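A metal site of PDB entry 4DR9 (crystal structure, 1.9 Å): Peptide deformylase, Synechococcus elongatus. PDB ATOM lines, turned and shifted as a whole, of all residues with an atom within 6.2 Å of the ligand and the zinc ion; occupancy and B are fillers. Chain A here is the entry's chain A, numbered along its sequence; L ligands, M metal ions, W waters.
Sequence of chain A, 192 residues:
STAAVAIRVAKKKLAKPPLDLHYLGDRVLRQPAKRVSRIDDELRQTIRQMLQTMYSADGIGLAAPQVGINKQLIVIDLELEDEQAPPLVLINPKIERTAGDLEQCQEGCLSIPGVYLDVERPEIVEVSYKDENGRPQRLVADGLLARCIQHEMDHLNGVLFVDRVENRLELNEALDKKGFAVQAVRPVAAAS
OE1 of Gln 66 is in hydrogen-bond range of N1 of the ligand, 3.3 Å away. The side-chain carboxylate (OE2) of Glu 152 sits at hydrogen-bond distance from a nitrogen (N1) of the ligand (2.6 Å). N of Gly 108 sits at hydrogen-bond distance from O4 of the ligand (2.6 Å). A nitrogen (N2) of the ligand sits at hydrogen-bond distance from the backbone carbonyl oxygen of Gly 108, at 3.2 Å. N of Ile 60 lies within hydrogen-bond range of O3 of the ligand, 2.9 Å away. An oxygen (O1) of the ligand sits close to the backbone NH of Leu 110, at 2.9 Å. A nitrogen (N1) of the ligand lies close to the backbone carbonyl oxygen (O) of Gly 61, 3.3 Å away.
A ring nitrogen (NE2) of His 155 lies close to the side-chain amide oxygen (OE1) of Gln 66 (3.4 Å). The side-chain carboxylate (OE1) of Glu 107 lies within hydrogen-bond range of a ring nitrogen (ND1) of His 151, 2.8 Å away. N of Ser 111 lies close to SG of Cys 109 (3.4 Å). The side-chain carboxylate (OE1) of Glu 152 lies close to the side-chain amide oxygen (OE1) of Gln 66, 3.5 Å away. The side-chain hydroxyl (OG) of Ser 111 is in hydrogen-bond range of the side-chain amide nitrogen (NE2) of Gln 66. OE1 of Gln 66 lies within hydrogen-bond range of N of Ala 63. The side-chain carboxylate (OE2) of Glu 107 lies within salt-bridge range of the guanidinium group (NH1) of Arg 147, 2.9 Å away. OE2 of Glu 107 lies within salt-bridge range of NE of Arg 121 (2.6 Å).
Residues that only touch the ligand: Gly 59 (3.5 Å), Glu 107 (3.7 Å), Leu 144 (3.8 Å), Gln 106 (3.8 Å) and Arg 147 (3.98 Å). Hydrophobic or aromatic side chains within 4 Å of the ligand: Ile 60, Leu 110, Leu 144, His 151 and His 155. 14 residues have an atom within 4 Å of the ligand: Gly 59, Ile 60, Gly 61, Gln 66, Gln 106, Glu 107, Gly 108, Cys 109, Leu 110, Leu 144, Arg 147, His 151, Glu 152 and His 155.
Gln 66 touches the zinc ion (NE2 to ZN, 3.5 Å). Of the 24 residues printed, 4 come within 4 Å of the zinc ion. The nearest printed residue that does not touch the zinc ion is Leu 110 (4.3 Å).
The zinc ion is bound by O1 of the ligand (2.1 Å), NE2 of His 155 (2.1 Å), NE2 of His 151 (2.1 Å), O2 of the ligand (2.2 Å) and SG of Cys 109 (2.3 Å).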
ATOM      1  N   ALA A  57      -9.075   5.436   4.173  1.00  0.00           N
ATOM      2  CA  ALA A  57     -10.552   5.417   3.943  1.00  0.00           C
ATOM      3  C   ALA A  57     -11.184   4.017   3.955  1.00  0.00           C
ATOM      4  O   ALA A  57     -12.386   3.871   3.697  1.00  0.00           O
ATOM      5  CB  ALA A  57     -10.885   6.083   2.622  1.00  0.00           C
ATOM      6  N   ASP A  58     -10.385   2.994   4.240  1.00  0.00           N
ATOM      7  CA  ASP A  58     -10.822   1.564   4.259  1.00  0.00           C
ATOM      8  C   ASP A  58     -11.382   1.017   2.956  1.00  0.00           C
ATOM      9  O   ASP A  58     -12.307   0.205   2.983  1.00  0.00           O
ATOM     10  CB  ASP A  58     -11.871   1.274   5.377  1.00  0.00           C
ATOM     11  CG  ASP A  58     -11.299   1.336   6.763  1.00  0.00           C
ATOM     12  OD1 ASP A  58     -10.276   0.633   7.066  1.00  0.00           O
ATOM     13  OD2 ASP A  58     -11.888   2.093   7.550  1.00  0.00           O
ATOM     14  N   GLY A  59     -10.851   1.445   1.831  1.00  0.00           N
ATOM     15  CA  GLY A  59     -11.270   0.932   0.543  1.00  0.00           C
ATOM     16  C   GLY A  59     -10.456  -0.269   0.160  1.00  0.00           C
ATOM     17  O   GLY A  59      -9.372  -0.486   0.741  1.00  0.00           O
ATOM     18  N   ILE A  60     -10.948  -1.031  -0.815  1.00  0.00           N
ATOM     19  CA  ILE A  60     -10.173  -2.137  -1.417  1.00  0.00           C
ATOM     20  C   ILE A  60      -9.608  -1.807  -2.799  1.00  0.00           C
ATOM     21  O   ILE A  60      -8.803  -2.556  -3.291  1.00  0.00           O
ATOM     22  CB  ILE A  60     -10.906  -3.508  -1.505  1.00  0.00           C
ATOM     23  CG1 ILE A  60     -12.056  -3.448  -2.494  1.00  0.00           C
ATOM     24  CG2 ILE A  60     -11.288  -3.975  -0.077  1.00  0.00           C
ATOM     25  CD1 ILE A  60     -12.854  -4.735  -2.662  1.00  0.00           C
ATOM     26  N   GLY A  61      -9.994  -0.652  -3.358  1.00  0.00           N
ATOM     27  CA  GLY A  61      -9.436  -0.159  -4.594  1.00  0.00           C
ATOM     28  C   GLY A  61      -9.581   1.339  -4.656  1.00  0.00           C
ATOM     29  O   GLY A  61     -10.356   1.939  -3.879  1.00  0.00           O
ATOM     30  N   LEU A  62      -8.830   1.958  -5.565  1.00  0.00           N
ATOM     31  CA  LEU A  62      -8.894   3.411  -5.768  1.00  0.00           C
ATOM     32  C   LEU A  62      -8.430   3.704  -7.185  1.00  0.00           C
ATOM     33  O   LEU A  62      -7.392   3.159  -7.627  1.00  0.00           O
ATOM     34  CB  LEU A  62      -8.047   4.209  -4.748  1.00  0.00           C
ATOM     35  CG  LEU A  62      -8.185   5.752  -4.739  1.00  0.00           C
ATOM     36  CD1 LEU A  62      -9.623   6.188  -4.442  1.00  0.00           C
ATOM     37  CD2 LEU A  62      -7.241   6.359  -3.697  1.00  0.00           C
ATOM     38  N   ALA A  63      -9.235   4.477  -7.920  1.00  0.00           N
ATOM     39  CA  ALA A  63      -8.903   4.930  -9.269  1.00  0.00           C
ATOM     40  C   ALA A  63      -8.508   6.390  -9.209  1.00  0.00           C
ATOM     41  O   ALA A  63      -9.114   7.169  -8.490  1.00  0.00           O
ATOM     42  CB  ALA A  63     -10.090   4.760 -10.240  1.00  0.00           C
ATOM     43  N   GLN A  66     -10.772   9.541  -8.859  1.00  0.00           N
ATOM     44  CA  GLN A  66     -11.448   9.755  -7.586  1.00  0.00           C
ATOM     45  C   GLN A  66     -10.715  10.733  -6.705  1.00  0.00           C
ATOM     46  O   GLN A  66     -11.312  11.350  -5.811  1.00  0.00           O
ATOM     47  CB  GLN A  66     -11.597   8.443  -6.814  1.00  0.00           C
ATOM     48  CG  GLN A  66     -12.454   7.404  -7.516  1.00  0.00           C
ATOM     49  CD  GLN A  66     -12.611   6.179  -6.671  1.00  0.00           C
ATOM     50  OE1 GLN A  66     -11.951   5.168  -6.934  1.00  0.00           O
ATOM     51  NE2 GLN A  66     -13.459   6.262  -5.601  1.00  0.00           N
ATOM     52  N   GLN A 106     -23.951  -6.321  -3.600  1.00  0.00           N
ATOM     53  CA  GLN A 106     -23.914  -4.988  -3.004  1.00  0.00           C
ATOM     54  C   GLN A 106     -22.587  -4.310  -3.258  1.00  0.00           C
ATOM     55  O   GLN A 106     -21.525  -4.938  -3.068  1.00  0.00           O
ATOM     56  CB  GLN A 106     -24.106  -5.144  -1.493  1.00  0.00           C
ATOM     57  CG  GLN A 106     -25.547  -5.407  -1.150  1.00  0.00           C
ATOM     58  CD  GLN A 106     -26.375  -4.128  -1.043  1.00  0.00           C
ATOM     59  OE1 GLN A 106     -27.254  -3.854  -1.890  1.00  0.00           O
ATOM     60  NE2 GLN A 106     -26.141  -3.376   0.034  1.00  0.00           N
ATOM     61  N   GLU A 107     -22.623  -3.076  -3.766  1.00  0.00           N
ATOM     62  CA  GLU A 107     -21.424  -2.277  -3.920  1.00  0.00           C
ATOM     63  C   GLU A 107     -21.502  -0.924  -3.221  1.00  0.00           C
ATOM     64  O   GLU A 107     -22.571  -0.357  -3.100  1.00  0.00           O
ATOM     65  CB  GLU A 107     -21.137  -2.015  -5.402  1.00  0.00           C
ATOM     66  CG  GLU A 107     -20.583  -3.226  -6.074  1.00  0.00           C
ATOM     67  CD  GLU A 107     -20.075  -2.932  -7.495  1.00  0.00           C
ATOM     68  OE1 GLU A 107     -19.598  -1.802  -7.769  1.00  0.00           O
ATOM     69  OE2 GLU A 107     -20.161  -3.858  -8.333  1.00  0.00           O
ATOM     70  N   GLY A 108     -20.381  -0.475  -2.712  1.00  0.00           N
ATOM     71  CA  GLY A 108     -20.187   0.899  -2.279  1.00  0.00           C
ATOM     72  C   GLY A 108     -18.987   1.522  -2.989  1.00  0.00           C
ATOM     73  O   GLY A 108     -18.270   0.842  -3.734  1.00  0.00           O
ATOM     74  N   CYS A 109     -18.772   2.818  -2.762  1.00  0.00           N
ATOM     75  CA  CYS A 109     -17.717   3.566  -3.449  1.00  0.00           C
ATOM     76  C   CYS A 109     -17.266   4.672  -2.518  1.00  0.00           C
ATOM     77  O   CYS A 109     -18.081   5.307  -1.859  1.00  0.00           O
ATOM     78  CB  CYS A 109     -18.253   4.124  -4.765  1.00  0.00           C
ATOM     79  SG  CYS A 109     -17.138   5.124  -5.792  1.00  0.00           S
ATOM     80  N   LEU A 110     -15.950   4.872  -2.447  1.00  0.00           N
ATOM     81  CA  LEU A 110     -15.388   5.941  -1.676  1.00  0.00           C
ATOM     82  C   LEU A 110     -15.840   7.317  -2.205  1.00  0.00           C
ATOM     83  O   LEU A 110     -15.883   8.291  -1.434  1.00  0.00           O
ATOM     84  CB  LEU A 110     -13.851   5.885  -1.705  1.00  0.00           C
ATOM     85  CG  LEU A 110     -13.208   4.655  -1.028  1.00  0.00           C
ATOM     86  CD1 LEU A 110     -11.701   4.656  -1.291  1.00  0.00           C
ATOM     87  CD2 LEU A 110     -13.473   4.644   0.462  1.00  0.00           C
ATOM     88  N   SER A 111     -16.220   7.406  -3.477  1.00  0.00           N
ATOM     89  CA  SER A 111     -16.768   8.645  -4.016  1.00  0.00           C
ATOM     90  C   SER A 111     -18.252   8.858  -3.738  1.00  0.00           C
ATOM     91  O   SER A 111     -18.814   9.938  -4.062  1.00  0.00           O
ATOM     92  CB  SER A 111     -16.482   8.720  -5.503  1.00  0.00           C
ATOM     93  OG  SER A 111     -15.101   8.902  -5.673  1.00  0.00           O
ATOM     94  N   TYR A 116     -25.016   1.980  -0.495  1.00  0.00           N
ATOM     95  CA  TYR A 116     -24.827   0.568  -0.846  1.00  0.00           C
ATOM     96  C   TYR A 116     -26.002   0.090  -1.663  1.00  0.00           C
ATOM     97  O   TYR A 116     -27.159   0.162  -1.222  1.00  0.00           O
ATOM     98  CB  TYR A 116     -24.557  -0.314   0.419  1.00  0.00           C
ATOM     99  CG  TYR A 116     -23.359   0.201   1.156  1.00  0.00           C
ATOM    100  CD1 TYR A 116     -22.072  -0.158   0.775  1.00  0.00           C
ATOM    101  CD2 TYR A 116     -23.508   1.118   2.187  1.00  0.00           C
ATOM    102  CE1 TYR A 116     -20.969   0.389   1.428  1.00  0.00           C
ATOM    103  CE2 TYR A 116     -22.432   1.651   2.847  1.00  0.00           C
ATOM    104  CZ  TYR A 116     -21.163   1.305   2.464  1.00  0.00           C
ATOM    105  OH  TYR A 116     -20.114   1.883   3.170  1.00  0.00           O
ATOM    106  N   ARG A 121     -22.873  -7.557 -12.481  1.00  0.00           N
ATOM    107  CA  ARG A 121     -21.669  -7.615 -13.321  1.00  0.00           C
ATOM    108  C   ARG A 121     -21.328  -9.045 -13.689  1.00  0.00           C
ATOM    109  O   ARG A 121     -21.682  -9.974 -12.963  1.00  0.00           O
ATOM    110  CB  ARG A 121     -20.447  -7.050 -12.598  1.00  0.00           C
ATOM    111  CG  ARG A 121     -20.584  -5.616 -12.132  1.00  0.00           C
ATOM    112  CD  ARG A 121     -19.276  -5.124 -11.514  1.00  0.00           C
ATOM    113  NE  ARG A 121     -19.391  -3.820 -10.829  1.00  0.00           N
ATOM    114  CZ  ARG A 121     -19.204  -2.639 -11.399  1.00  0.00           C
ATOM    115  NH1 ARG A 121     -18.920  -2.515 -12.687  1.00  0.00           N
ATOM    116  NH2 ARG A 121     -19.320  -1.544 -10.695  1.00  0.00           N
ATOM    117  N   LEU A 144     -14.679 -11.156  -5.650  1.00  0.00           N
ATOM    118  CA  LEU A 144     -14.582  -9.760  -5.235  1.00  0.00           C
ATOM    119  C   LEU A 144     -13.498  -9.034  -5.991  1.00  0.00           C
ATOM    120  O   LEU A 144     -13.709  -7.916  -6.389  1.00  0.00           O
ATOM    121  CB  LEU A 144     -14.328  -9.660  -3.703  1.00  0.00           C
ATOM    122  CG  LEU A 144     -14.155  -8.302  -3.051  1.00  0.00           C
ATOM    123  CD1 LEU A 144     -15.337  -7.383  -3.400  1.00  0.00           C
ATOM    124  CD2 LEU A 144     -13.922  -8.516  -1.533  1.00  0.00           C
ATOM    125  N   ARG A 147     -14.915  -8.059  -9.374  1.00  0.00           N
ATOM    126  CA  ARG A 147     -15.871  -7.009  -9.132  1.00  0.00           C
ATOM    127  C   ARG A 147     -15.159  -5.648  -8.952  1.00  0.00           C
ATOM    128  O   ARG A 147     -15.557  -4.667  -9.540  1.00  0.00           O
ATOM    129  CB  ARG A 147     -16.758  -7.320  -7.934  1.00  0.00           C
ATOM    130  CG  ARG A 147     -17.857  -6.289  -7.689  1.00  0.00           C
ATOM    131  CD  ARG A 147     -19.029  -6.791  -6.864  1.00  0.00           C
ATOM    132  NE  ARG A 147     -19.794  -7.811  -7.542  1.00  0.00           N
ATOM    133  CZ  ARG A 147     -20.897  -7.612  -8.269  1.00  0.00           C
ATOM    134  NH1 ARG A 147     -21.486  -6.424  -8.354  1.00  0.00           N
ATOM    135  NH2 ARG A 147     -21.465  -8.654  -8.842  1.00  0.00           N
ATOM    136  N   CYS A 148     -14.139  -5.615  -8.103  1.00  0.00           N
ATOM    137  CA  CYS A 148     -13.406  -4.395  -7.839  1.00  0.00           C
ATOM    138  C   CYS A 148     -12.736  -3.904  -9.125  1.00  0.00           C
ATOM    139  O   CYS A 148     -12.757  -2.721  -9.414  1.00  0.00           O
ATOM    140  CB  CYS A 148     -12.344  -4.694  -6.810  1.00  0.00           C
ATOM    141  SG  CYS A 148     -11.314  -3.306  -6.380  1.00  0.00           S
ATOM    142  N   HIS A 151     -15.320  -2.295 -11.298  1.00  0.00           N
ATOM    143  CA  HIS A 151     -15.663  -1.013 -10.646  1.00  0.00           C
ATOM    144  C   HIS A 151     -14.630   0.044 -10.866  1.00  0.00           C
ATOM    145  O   HIS A 151     -14.945   1.203 -11.182  1.00  0.00           O
ATOM    146  CB  HIS A 151     -15.931  -1.296  -9.168  1.00  0.00           C
ATOM    147  CG  HIS A 151     -16.268  -0.094  -8.351  1.00  0.00           C
ATOM    148  ND1 HIS A 151     -17.452   0.031  -7.696  1.00  0.00           N
ATOM    149  CD2 HIS A 151     -15.518   1.010  -8.005  1.00  0.00           C
ATOM    150  CE1 HIS A 151     -17.460   1.153  -6.982  1.00  0.00           C
ATOM    151  NE2 HIS A 151     -16.283   1.757  -7.143  1.00  0.00           N
ATOM    152  N   GLU A 152     -13.374  -0.305 -10.689  1.00  0.00           N
ATOM    153  CA  GLU A 152     -12.302   0.664 -10.912  1.00  0.00           C
ATOM    154  C   GLU A 152     -12.131   1.078 -12.381  1.00  0.00           C
ATOM    155  O   GLU A 152     -11.902   2.262 -12.684  1.00  0.00           O
ATOM    156  CB  GLU A 152     -10.982   0.141 -10.377  1.00  0.00           C
ATOM    157  CG  GLU A 152     -11.018  -0.297  -8.911  1.00  0.00           C
ATOM    158  CD  GLU A 152     -11.476   0.776  -7.957  1.00  0.00           C
ATOM    159  OE1 GLU A 152     -11.480   1.979  -8.289  1.00  0.00           O
ATOM    160  OE2 GLU A 152     -11.830   0.443  -6.832  1.00  0.00           O
ATOM    161  N   HIS A 155     -14.511   3.729 -13.294  1.00  0.00           N
ATOM    162  CA  HIS A 155     -14.058   5.067 -12.890  1.00  0.00           C
ATOM    163  C   HIS A 155     -13.158   5.660 -13.938  1.00  0.00           C
ATOM    164  O   HIS A 155     -13.204   6.838 -14.122  1.00  0.00           O
ATOM    165  CB  HIS A 155     -13.243   5.064 -11.564  1.00  0.00           C
ATOM    166  CG  HIS A 155     -14.062   4.990 -10.308  1.00  0.00           C
ATOM    167  ND1 HIS A 155     -14.906   5.969  -9.924  1.00  0.00           N
ATOM    168  CD2 HIS A 155     -14.109   4.031  -9.328  1.00  0.00           C
ATOM    169  CE1 HIS A 155     -15.463   5.645  -8.761  1.00  0.00           C
ATOM    170  NE2 HIS A 155     -14.969   4.454  -8.387  1.00  0.00           N
ATOM    171  N   LEU A 160     -19.870   5.443 -12.799  1.00  0.00           N
ATOM    172  CA  LEU A 160     -20.019   5.194 -11.373  1.00  0.00           C
ATOM    173  C   LEU A 160     -21.055   4.137 -11.178  1.00  0.00           C
ATOM    174  O   LEU A 160     -21.962   3.984 -12.013  1.00  0.00           O
ATOM    175  CB  LEU A 160     -20.420   6.481 -10.637  1.00  0.00           C
ATOM    176  CG  LEU A 160     -19.486   7.669 -10.778  1.00  0.00           C
ATOM    177  CD1 LEU A 160     -20.047   8.927 -10.157  1.00  0.00           C
ATOM    178  CD2 LEU A 160     -18.099   7.352 -10.166  1.00  0.00           C
ATOM    179  N   PHE A 161     -20.951   3.395 -10.080  1.00  0.00           N
ATOM    180  CA  PHE A 161     -21.757   2.207  -9.875  1.00  0.00           C
ATOM    181  C   PHE A 161     -23.242   2.477  -9.854  1.00  0.00           C
ATOM    182  O   PHE A 161     -24.031   1.622 -10.299  1.00  0.00           O
ATOM    183  CB  PHE A 161     -21.285   1.384  -8.675  1.00  0.00           C
ATOM    184  CG  PHE A 161     -21.812   1.839  -7.333  1.00  0.00           C
ATOM    185  CD1 PHE A 161     -21.122   2.818  -6.611  1.00  0.00           C
ATOM    186  CD2 PHE A 161     -22.999   1.334  -6.823  1.00  0.00           C
ATOM    187  CE1 PHE A 161     -21.588   3.245  -5.375  1.00  0.00           C
ATOM    188  CE2 PHE A 161     -23.461   1.774  -5.591  1.00  0.00           C
ATOM    189  CZ  PHE A 161     -22.763   2.715  -4.883  1.00  0.00           C
HETATM  190  C1  LIG L   1     -13.569   1.688  -3.401  1.00  0.00           C
HETATM  191  C2  LIG L   1     -13.831   2.576  -4.589  1.00  0.00           C
HETATM  192  O1  LIG L   1     -14.704   3.419  -4.682  1.00  0.00           O
HETATM  193  N1  LIG L   1     -13.116   2.348  -5.628  1.00  0.00           N
HETATM  194  O2  LIG L   1     -13.356   3.191  -6.675  1.00  0.00           O
HETATM  195  C3  LIG L   1     -14.474   0.456  -3.540  1.00  0.00           C
HETATM  196  C4  LIG L   1     -14.664  -0.113  -2.164  1.00  0.00           C
HETATM  197  O3  LIG L   1     -13.720  -0.470  -1.494  1.00  0.00           O
HETATM  198  C5  LIG L   1     -13.875  -0.583  -4.479  1.00  0.00           C
HETATM  199  C6  LIG L   1     -14.618  -1.945  -4.565  1.00  0.00           C
HETATM  200  C7  LIG L   1     -16.019  -1.816  -5.107  1.00  0.00           C
HETATM  201  C8  LIG L   1     -16.543  -3.167  -5.594  1.00  0.00           C
HETATM  202  C9  LIG L   1     -17.256  -3.899  -4.475  1.00  0.00           C
HETATM  203  N2  LIG L   1     -15.927  -0.213  -1.753  1.00  0.00           N
HETATM  204  C10 LIG L   1     -16.342  -0.854  -0.515  1.00  0.00           C
HETATM  205  C11 LIG L   1     -16.915   0.194   0.450  1.00  0.00           C
HETATM  206  C12 LIG L   1     -16.953  -0.325   1.877  1.00  0.00           C
HETATM  207  C13 LIG L   1     -16.091   1.478   0.439  1.00  0.00           C
HETATM  208  C14 LIG L   1     -17.357  -1.923  -0.848  1.00  0.00           C
HETATM  209  O4  LIG L   1     -18.409  -1.585  -1.359  1.00  0.00           O
HETATM  210  N3  LIG L   1     -17.154  -3.198  -0.610  1.00  0.00           N
HETATM  211  C15 LIG L   1     -18.242  -4.146  -0.845  1.00  0.00           C
HETATM  212  C16 LIG L   1     -15.916  -3.800  -0.158  1.00  0.00           C
HETATM  213  C17 LIG L   1     -16.163  -5.281  -0.391  1.00  0.00           C
HETATM  214  C18 LIG L   1     -17.653  -5.504  -0.498  1.00  0.00           C
HETATM  215  C19 LIG L   1     -19.486  -3.862   0.014  1.00  0.00           C
HETATM  216  O5  LIG L   1     -19.213  -4.110   1.391  1.00  0.00           O
HETATM  217 ZN    ZN M   1     -15.511   3.653  -6.557  1.00  0.00          ZN
HETATM  218  O   HOH W   1     -19.045  -2.502   3.209  1.00  0.00           O
HETATM  219  O   HOH W   2     -20.505  -6.531   2.266  1.00  0.00           O
